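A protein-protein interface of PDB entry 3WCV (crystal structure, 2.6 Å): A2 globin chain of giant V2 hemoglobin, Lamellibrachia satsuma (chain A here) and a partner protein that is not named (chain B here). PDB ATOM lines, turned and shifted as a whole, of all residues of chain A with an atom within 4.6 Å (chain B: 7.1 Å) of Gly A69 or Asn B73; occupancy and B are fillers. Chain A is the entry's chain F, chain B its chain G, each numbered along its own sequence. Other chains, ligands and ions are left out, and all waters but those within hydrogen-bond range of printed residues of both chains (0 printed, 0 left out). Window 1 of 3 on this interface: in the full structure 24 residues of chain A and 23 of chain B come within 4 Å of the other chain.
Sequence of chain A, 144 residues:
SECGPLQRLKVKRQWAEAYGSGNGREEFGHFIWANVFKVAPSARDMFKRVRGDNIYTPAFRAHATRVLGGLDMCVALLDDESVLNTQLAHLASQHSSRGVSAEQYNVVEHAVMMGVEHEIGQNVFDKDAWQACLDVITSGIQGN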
ATOM      1  N   TYR A  19     -38.962 -13.707  31.941  1.00  0.00           N
ATOM      2  CA  TYR A  19     -37.957 -13.314  30.976  1.00  0.00           C
ATOM      3  C   TYR A  19     -38.462 -13.673  29.573  1.00  0.00           C
ATOM      4  O   TYR A  19     -38.280 -12.924  28.611  1.00  0.00           O
ATOM      5  CB  TYR A  19     -36.650 -14.030  31.317  1.00  0.00           C
ATOM      6  CG  TYR A  19     -35.421 -13.543  30.587  1.00  0.00           C
ATOM      7  CD1 TYR A  19     -35.183 -12.174  30.398  1.00  0.00           C
ATOM      8  CD2 TYR A  19     -34.469 -14.455  30.123  1.00  0.00           C
ATOM      9  CE1 TYR A  19     -34.016 -11.727  29.756  1.00  0.00           C
ATOM     10  CE2 TYR A  19     -33.310 -14.029  29.487  1.00  0.00           C
ATOM     11  CZ  TYR A  19     -33.088 -12.669  29.307  1.00  0.00           C
ATOM     12  OH  TYR A  19     -31.934 -12.253  28.677  1.00  0.00           O
ATOM     13  N   THR A  65     -30.179  -5.090  28.645  1.00  0.00           N
ATOM     14  CA  THR A  65     -30.119  -6.369  27.959  1.00  0.00           C
ATOM     15  C   THR A  65     -28.998  -7.194  28.589  1.00  0.00           C
ATOM     16  O   THR A  65     -29.158  -8.389  28.856  1.00  0.00           O
ATOM     17  CB  THR A  65     -29.793  -6.203  26.457  1.00  0.00           C
ATOM     18  OG1 THR A  65     -30.904  -5.606  25.784  1.00  0.00           O
ATOM     19  CG2 THR A  65     -29.475  -7.565  25.815  1.00  0.00           C
ATOM     20  N   ARG A  66     -27.859  -6.541  28.818  1.00  0.00           N
ATOM     21  CA  ARG A  66     -26.717  -7.208  29.410  1.00  0.00           C
ATOM     22  C   ARG A  66     -27.017  -7.619  30.849  1.00  0.00           C
ATOM     23  O   ARG A  66     -26.735  -8.749  31.242  1.00  0.00           O
ATOM     24  CB  ARG A  66     -25.478  -6.300  29.374  1.00  0.00           C
ATOM     25  CG  ARG A  66     -24.899  -6.044  27.984  1.00  0.00           C
ATOM     26  CD  ARG A  66     -23.574  -5.295  28.084  1.00  0.00           C
ATOM     27  NE  ARG A  66     -23.706  -3.865  28.364  1.00  0.00           N
ATOM     28  CZ  ARG A  66     -23.927  -2.942  27.434  1.00  0.00           C
ATOM     29  NH1 ARG A  66     -24.033  -1.662  27.767  1.00  0.00           N
ATOM     30  NH2 ARG A  66     -24.045  -3.293  26.160  1.00  0.00           N
ATOM     31  N   VAL A  67     -27.594  -6.719  31.637  1.00  0.00           N
ATOM     32  CA  VAL A  67     -27.894  -7.061  33.018  1.00  0.00           C
ATOM     33  C   VAL A  67     -28.788  -8.309  33.090  1.00  0.00           C
ATOM     34  O   VAL A  67     -28.382  -9.333  33.651  1.00  0.00           O
ATOM     35  CB  VAL A  67     -28.594  -5.908  33.762  1.00  0.00           C
ATOM     36  CG1 VAL A  67     -28.867  -6.309  35.205  1.00  0.00           C
ATOM     37  CG2 VAL A  67     -27.737  -4.671  33.704  1.00  0.00           C
ATOM     38  N   LEU A  68     -29.991  -8.227  32.516  1.00  0.00           N
ATOM     39  CA  LEU A  68     -30.921  -9.347  32.528  1.00  0.00           C
ATOM     40  C   LEU A  68     -30.238 -10.632  32.045  1.00  0.00           C
ATOM     41  O   LEU A  68     -30.476 -11.707  32.608  1.00  0.00           O
ATOM     42  CB  LEU A  68     -32.149  -9.020  31.669  1.00  0.00           C
ATOM     43  CG  LEU A  68     -32.952  -7.762  32.055  1.00  0.00           C
ATOM     44  CD1 LEU A  68     -34.382  -7.864  31.519  1.00  0.00           C
ATOM     45  CD2 LEU A  68     -32.985  -7.613  33.565  1.00  0.00           C
ATOM     46  N   GLY A  69     -29.391 -10.512  31.019  1.00  0.00           N
ATOM     47  CA  GLY A  69     -28.666 -11.667  30.506  1.00  0.00           C
ATOM     48  C   GLY A  69     -27.772 -12.224  31.606  1.00  0.00           C
ATOM     49  O   GLY A  69     -27.584 -13.445  31.723  1.00  0.00           O
ATOM     50  N   GLY A  70     -27.214 -11.315  32.407  1.00  0.00           N
ATOM     51  CA  GLY A  70     -26.367 -11.713  33.511  1.00  0.00           C
ATOM     52  C   GLY A  70     -27.217 -12.526  34.465  1.00  0.00           C
ATOM     53  O   GLY A  70     -26.855 -13.646  34.823  1.00  0.00           O
ATOM     54  N   LEU A  71     -28.357 -11.968  34.872  1.00  0.00           N
ATOM     55  CA  LEU A  71     -29.272 -12.673  35.771  1.00  0.00           C
ATOM     56  C   LEU A  71     -29.611 -14.040  35.204  1.00  0.00           C
ATOM     57  O   LEU A  71     -29.501 -15.044  35.890  1.00  0.00           O
ATOM     58  CB  LEU A  71     -30.573 -11.887  35.947  1.00  0.00           C
ATOM     59  CG  LEU A  71     -30.606 -10.849  37.061  1.00  0.00           C
ATOM     60  CD1 LEU A  71     -31.899 -10.037  37.013  1.00  0.00           C
ATOM     61  CD2 LEU A  71     -30.480 -11.575  38.384  1.00  0.00           C
ATOM     62  N   ASP A  72     -30.020 -14.066  33.939  1.00  0.00           N
ATOM     63  CA  ASP A  72     -30.392 -15.305  33.304  1.00  0.00           C
ATOM     64  C   ASP A  72     -29.328 -16.372  33.496  1.00  0.00           C
ATOM     65  O   ASP A  72     -29.648 -17.504  33.880  1.00  0.00           O
ATOM     66  CB  ASP A  72     -30.642 -15.077  31.824  1.00  0.00           C
ATOM     67  CG  ASP A  72     -31.162 -16.308  31.135  1.00  0.00           C
ATOM     68  OD1 ASP A  72     -30.377 -16.966  30.420  1.00  0.00           O
ATOM     69  OD2 ASP A  72     -32.357 -16.624  31.324  1.00  0.00           O
ATOM     70  N   MET A  73     -28.069 -16.017  33.248  1.00  0.00           N
ATOM     71  CA  MET A  73     -26.989 -16.994  33.397  1.00  0.00           C
ATOM     72  C   MET A  73     -26.933 -17.559  34.807  1.00  0.00           C
ATOM     73  O   MET A  73     -26.773 -18.757  34.985  1.00  0.00           O
ATOM     74  CB  MET A  73     -25.640 -16.385  32.989  1.00  0.00           C
ATOM     75  CG  MET A  73     -25.579 -16.051  31.503  1.00  0.00           C
ATOM     76  SD  MET A  73     -23.959 -15.589  30.841  1.00  0.00           S
ATOM     77  CE  MET A  73     -23.872 -13.902  31.442  1.00  0.00           C
ATOM     78  N   TRP B  17     -33.288 -20.484  16.664  1.00  0.00           N
ATOM     79  CA  TRP B  17     -32.605 -20.347  17.937  1.00  0.00           C
ATOM     80  C   TRP B  17     -33.465 -20.872  19.076  1.00  0.00           C
ATOM     81  O   TRP B  17     -33.137 -21.892  19.668  1.00  0.00           O
ATOM     82  CB  TRP B  17     -32.239 -18.881  18.168  1.00  0.00           C
ATOM     83  CG  TRP B  17     -31.308 -18.642  19.311  1.00  0.00           C
ATOM     84  CD1 TRP B  17     -31.551 -17.903  20.441  1.00  0.00           C
ATOM     85  CD2 TRP B  17     -29.989 -19.171  19.450  1.00  0.00           C
ATOM     86  NE1 TRP B  17     -30.460 -17.948  21.277  1.00  0.00           N
ATOM     87  CE2 TRP B  17     -29.488 -18.722  20.691  1.00  0.00           C
ATOM     88  CE3 TRP B  17     -29.178 -19.986  18.640  1.00  0.00           C
ATOM     89  CZ2 TRP B  17     -28.211 -19.067  21.146  1.00  0.00           C
ATOM     90  CZ3 TRP B  17     -27.913 -20.326  19.088  1.00  0.00           C
ATOM     91  CH2 TRP B  17     -27.441 -19.868  20.332  1.00  0.00           C
ATOM     92  N   TRP B  21     -32.821 -23.511  22.572  1.00  0.00           N
ATOM     93  CA  TRP B  21     -32.377 -22.568  23.587  1.00  0.00           C
ATOM     94  C   TRP B  21     -33.255 -22.689  24.825  1.00  0.00           C
ATOM     95  O   TRP B  21     -34.212 -21.941  24.977  1.00  0.00           O
ATOM     96  CB  TRP B  21     -32.463 -21.150  23.040  1.00  0.00           C
ATOM     97  CG  TRP B  21     -31.903 -20.106  23.963  1.00  0.00           C
ATOM     98  CD1 TRP B  21     -30.607 -19.660  24.028  1.00  0.00           C
ATOM     99  CD2 TRP B  21     -32.617 -19.400  24.978  1.00  0.00           C
ATOM    100  NE1 TRP B  21     -30.473 -18.717  25.031  1.00  0.00           N
ATOM    101  CE2 TRP B  21     -31.693 -18.539  25.629  1.00  0.00           C
ATOM    102  CE3 TRP B  21     -33.947 -19.411  25.407  1.00  0.00           C
ATOM    103  CZ2 TRP B  21     -32.066 -17.697  26.686  1.00  0.00           C
ATOM    104  CZ3 TRP B  21     -34.318 -18.572  26.464  1.00  0.00           C
ATOM    105  CH2 TRP B  21     -33.378 -17.729  27.089  1.00  0.00           C
ATOM    106  N   ARG B  29     -27.701 -25.361  26.278  1.00  0.00           N
ATOM    107  CA  ARG B  29     -26.875 -24.222  25.877  1.00  0.00           C
ATOM    108  C   ARG B  29     -25.404 -24.622  25.793  1.00  0.00           C
ATOM    109  O   ARG B  29     -24.705 -24.331  24.816  1.00  0.00           O
ATOM    110  CB  ARG B  29     -27.013 -23.083  26.891  1.00  0.00           C
ATOM    111  CG  ARG B  29     -28.416 -22.665  27.186  1.00  0.00           C
ATOM    112  CD  ARG B  29     -28.416 -21.479  28.120  1.00  0.00           C
ATOM    113  NE  ARG B  29     -29.762 -21.119  28.542  1.00  0.00           N
ATOM    114  CZ  ARG B  29     -30.035 -20.084  29.325  1.00  0.00           C
ATOM    115  NH1 ARG B  29     -29.049 -19.310  29.760  1.00  0.00           N
ATOM    116  NH2 ARG B  29     -31.289 -19.817  29.665  1.00  0.00           N
ATOM    117  N   HIS B  67     -17.427 -19.654  30.210  1.00  0.00           N
ATOM    118  CA  HIS B  67     -17.173 -18.872  29.013  1.00  0.00           C
ATOM    119  C   HIS B  67     -18.169 -19.257  27.928  1.00  0.00           C
ATOM    120  O   HIS B  67     -18.661 -18.407  27.193  1.00  0.00           O
ATOM    121  CB  HIS B  67     -15.763 -19.092  28.484  1.00  0.00           C
ATOM    122  CG  HIS B  67     -15.544 -18.483  27.134  1.00  0.00           C
ATOM    123  ND1 HIS B  67     -15.561 -17.121  26.925  1.00  0.00           N
ATOM    124  CD2 HIS B  67     -15.384 -19.052  25.917  1.00  0.00           C
ATOM    125  CE1 HIS B  67     -15.417 -16.880  25.633  1.00  0.00           C
ATOM    126  NE2 HIS B  67     -15.309 -18.035  24.999  1.00  0.00           N
ATOM    127  N   CYS B  68     -18.456 -20.548  27.815  1.00  0.00           N
ATOM    128  CA  CYS B  68     -19.406 -21.009  26.812  1.00  0.00           C
ATOM    129  C   CYS B  68     -20.784 -20.381  27.034  1.00  0.00           C
ATOM    130  O   CYS B  68     -21.408 -19.890  26.093  1.00  0.00           O
ATOM    131  CB  CYS B  68     -19.500 -22.532  26.857  1.00  0.00           C
ATOM    132  SG  CYS B  68     -18.220 -23.359  25.880  1.00  0.00           S
ATOM    133  N   ILE B  69     -21.235 -20.392  28.286  1.00  0.00           N
ATOM    134  CA  ILE B  69     -22.527 -19.830  28.655  1.00  0.00           C
ATOM    135  C   ILE B  69     -22.555 -18.341  28.351  1.00  0.00           C
ATOM    136  O   ILE B  69     -23.583 -17.806  27.904  1.00  0.00           O
ATOM    137  CB  ILE B  69     -22.816 -20.057  30.150  1.00  0.00           C
ATOM    138  CG1 ILE B  69     -23.160 -21.527  30.371  1.00  0.00           C
ATOM    139  CG2 ILE B  69     -23.948 -19.145  30.634  1.00  0.00           C
ATOM    140  CD1 ILE B  69     -23.430 -21.880  31.814  1.00  0.00           C
ATOM    141  N   ARG B  70     -21.420 -17.682  28.585  1.00  0.00           N
ATOM    142  CA  ARG B  70     -21.300 -16.246  28.327  1.00  0.00           C
ATOM    143  C   ARG B  70     -21.401 -15.940  26.831  1.00  0.00           C
ATOM    144  O   ARG B  70     -21.975 -14.920  26.420  1.00  0.00           O
ATOM    145  CB  ARG B  70     -19.980 -15.690  28.897  1.00  0.00           C
ATOM    146  CG  ARG B  70     -20.013 -15.396  30.409  1.00  0.00           C
ATOM    147  CD  ARG B  70     -18.857 -14.490  30.886  1.00  0.00           C
ATOM    148  NE  ARG B  70     -17.531 -15.092  30.748  1.00  0.00           N
ATOM    149  CZ  ARG B  70     -17.041 -16.058  31.528  1.00  0.00           C
ATOM    150  NH1 ARG B  70     -17.751 -16.560  32.531  1.00  0.00           N
ATOM    151  NH2 ARG B  70     -15.825 -16.535  31.289  1.00  0.00           N
ATOM    152  N   VAL B  71     -20.844 -16.825  26.015  1.00  0.00           N
ATOM    153  CA  VAL B  71     -20.889 -16.644  24.574  1.00  0.00           C
ATOM    154  C   VAL B  71     -22.326 -16.778  24.055  1.00  0.00           C
ATOM    155  O   VAL B  71     -22.849 -15.840  23.429  1.00  0.00           O
ATOM    156  CB  VAL B  71     -19.963 -17.663  23.843  1.00  0.00           C
ATOM    157  CG1 VAL B  71     -20.079 -17.492  22.325  1.00  0.00           C
ATOM    158  CG2 VAL B  71     -18.519 -17.448  24.264  1.00  0.00           C
ATOM    159  N   VAL B  72     -22.972 -17.923  24.321  1.00  0.00           N
ATOM    160  CA  VAL B  72     -24.338 -18.097  23.834  1.00  0.00           C
ATOM    161  C   VAL B  72     -25.259 -17.010  24.373  1.00  0.00           C
ATOM    162  O   VAL B  72     -26.145 -16.539  23.648  1.00  0.00           O
ATOM    163  CB  VAL B  72     -24.940 -19.521  24.132  1.00  0.00           C
ATOM    164  CG1 VAL B  72     -24.207 -20.556  23.323  1.00  0.00           C
ATOM    165  CG2 VAL B  72     -24.865 -19.856  25.598  1.00  0.00           C
ATOM    166  N   ASN B  73     -25.044 -16.595  25.625  1.00  0.00           N
ATOM    167  CA  ASN B  73     -25.865 -15.535  26.201  1.00  0.00           C
ATOM    168  C   ASN B  73     -25.675 -14.292  25.354  1.00  0.00           C
ATOM    169  O   ASN B  73     -26.583 -13.470  25.207  1.00  0.00           O
ATOM    170  CB  ASN B  73     -25.441 -15.221  27.640  1.00  0.00           C
ATOM    171  CG  ASN B  73     -26.166 -13.989  28.220  1.00  0.00           C
ATOM    172  OD1 ASN B  73     -27.334 -14.063  28.610  1.00  0.00           O
ATOM    173  ND2 ASN B  73     -25.472 -12.852  28.266  1.00  0.00           N
ATOM    174  N   GLY B  74     -24.474 -14.162  24.792  1.00  0.00           N
ATOM    175  CA  GLY B  74     -24.158 -13.003  23.982  1.00  0.00           C
ATOM    176  C   GLY B  74     -24.809 -13.042  22.625  1.00  0.00           C
ATOM    177  O   GLY B  74     -25.261 -12.024  22.110  1.00  0.00           O
ATOM    178  N   LEU B  75     -24.831 -14.227  22.033  1.00  0.00           N
ATOM    179  CA  LEU B  75     -25.431 -14.413  20.722  1.00  0.00           C
ATOM    180  C   LEU B  75     -26.943 -14.321  20.901  1.00  0.00           C
ATOM    181  O   LEU B  75     -27.637 -13.759  20.055  1.00  0.00           O
ATOM    182  CB  LEU B  75     -25.040 -15.782  20.150  1.00  0.00           C
ATOM    183  CG  LEU B  75     -25.740 -16.204  18.852  1.00  0.00           C
ATOM    184  CD1 LEU B  75     -25.491 -15.188  17.767  1.00  0.00           C
ATOM    185  CD2 LEU B  75     -25.250 -17.585  18.416  1.00  0.00           C
ATOM    186  N   ASP B  76     -27.436 -14.877  22.011  1.00  0.00           N
ATOM    187  CA  ASP B  76     -28.862 -14.839  22.313  1.00  0.00           C
ATOM    188  C   ASP B  76     -29.333 -13.402  22.397  1.00  0.00           C
ATOM    189  O   ASP B  76     -30.364 -13.064  21.842  1.00  0.00           O
ATOM    190  CB  ASP B  76     -29.171 -15.546  23.637  1.00  0.00           C
ATOM    191  CG  ASP B  76     -30.635 -15.431  24.031  1.00  0.00           C
ATOM    192  OD1 ASP B  76     -30.952 -14.667  24.963  1.00  0.00           O
ATOM    193  OD2 ASP B  76     -31.479 -16.099  23.399  1.00  0.00           O
ATOM    194  N   SER B  77     -28.582 -12.554  23.088  1.00  0.00           N
ATOM    195  CA  SER B  77     -28.959 -11.156  23.214  1.00  0.00           C
ATOM    196  C   SER B  77     -28.950 -10.507  21.840  1.00  0.00           C
ATOM    197  O   SER B  77     -29.755  -9.622  21.563  1.00  0.00           O
ATOM    198  CB  SER B  77     -28.005 -10.407  24.153  1.00  0.00           C
ATOM    199  OG  SER B  77     -26.739 -10.153  23.552  1.00  0.00           O
ATOM    200  N   ALA B  78     -28.051 -10.951  20.970  1.00  0.00           N
ATOM    201  CA  ALA B  78     -27.972 -10.371  19.635  1.00  0.00           C
ATOM    202  C   ALA B  78     -29.114 -10.851  18.754  1.00  0.00           C
ATOM    203  O   ALA B  78     -29.735 -10.062  18.033  1.00  0.00           O
ATOM    204  CB  ALA B  78     -26.623 -10.713  18.985  1.00  0.00           C
ATOM    205  N   GLN B  91     -25.426  -2.867  21.552  1.00  0.00           N
ATOM    206  CA  GLN B  91     -24.990  -4.138  22.110  1.00  0.00           C
ATOM    207  C   GLN B  91     -23.823  -4.746  21.345  1.00  0.00           C
ATOM    208  O   GLN B  91     -22.932  -5.336  21.951  1.00  0.00           O
ATOM    209  CB  GLN B  91     -26.161  -5.125  22.122  1.00  0.00           C
ATOM    210  CG  GLN B  91     -25.812  -6.524  22.573  1.00  0.00           C
ATOM    211  CD  GLN B  91     -25.413  -6.578  24.029  1.00  0.00           C
ATOM    212  OE1 GLN B  91     -25.597  -5.612  24.778  1.00  0.00           O
ATOM    213  NE2 GLN B  91     -24.881  -7.719  24.450  1.00  0.00           N
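The side-chain amide oxygen of Gln B91 is in hydrogen-bond range of the guanidinium group of Arg A66 (3.1 Å). The side-chain amide oxygen (OD1) of Asn B73 sits close to the backbone carbonyl oxygen (O) of Gly A69. OD1 of Asp A72 lies within salt-bridge range of NH1 of Arg B29 (2.8 Å). The backbone carbonyl oxygen (O) of Ile B69 sits close to the side-chain sulfur (SD) of Met A73.
The backbone carbonyl oxygen (O) of Gly B74 sits at hydrogen-bond distance from the side-chain hydroxyl (OG) of Ser B77. The side-chain hydroxyl of Ser B77 lies within hydrogen-bond range of the side-chain amide nitrogen of Gln B91 (3.2 Å).
Thr A65 touches Ser B77 (CG2 to CB, 3.6 Å). Met A73 touches Arg B70. SD of Met A73 touches CB of Asn B73, 3.5 Å away.
Of chain B, only Asn B73 (3.2 Å) comes within 4 Å of Gly A69. Of the printed residues of chain B, Asp A72 touches Arg B29. Of the printed residues of chain B, Met A73 touches Ile B69 (3.6 Å), Arg B70 (3.7 Å) and Asn B73 (3.5 Å). Printed residues of chain A within 4 Å of Ser B77: Thr A65. Printed residues of chain A within 4 Å of Gln B91: Arg A66 (3.1 Å). The nearest residue of chain B that does not touch Gly A69 is Arg B29 (6.4 Å). The nearest printed residue of chain A that does not touch Asn B73 is Asp A72 (4.6 Å).
Of the 10 printed residues of chain A, 5 touch a printed residue of chain B. Printed residues of chain A that touch a printed residue of chain B: Thr A65, Arg A66, Gly A69, Asp A72 and Met A73. Among the printed residues, 7 pairs touch across the chains. Among the printed residues, Asp or Glu carboxylates within 4 Å of a Lys or Arg side-chain nitrogen of the other chain: Asp A72 with Arg B29 (2.8 Å).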
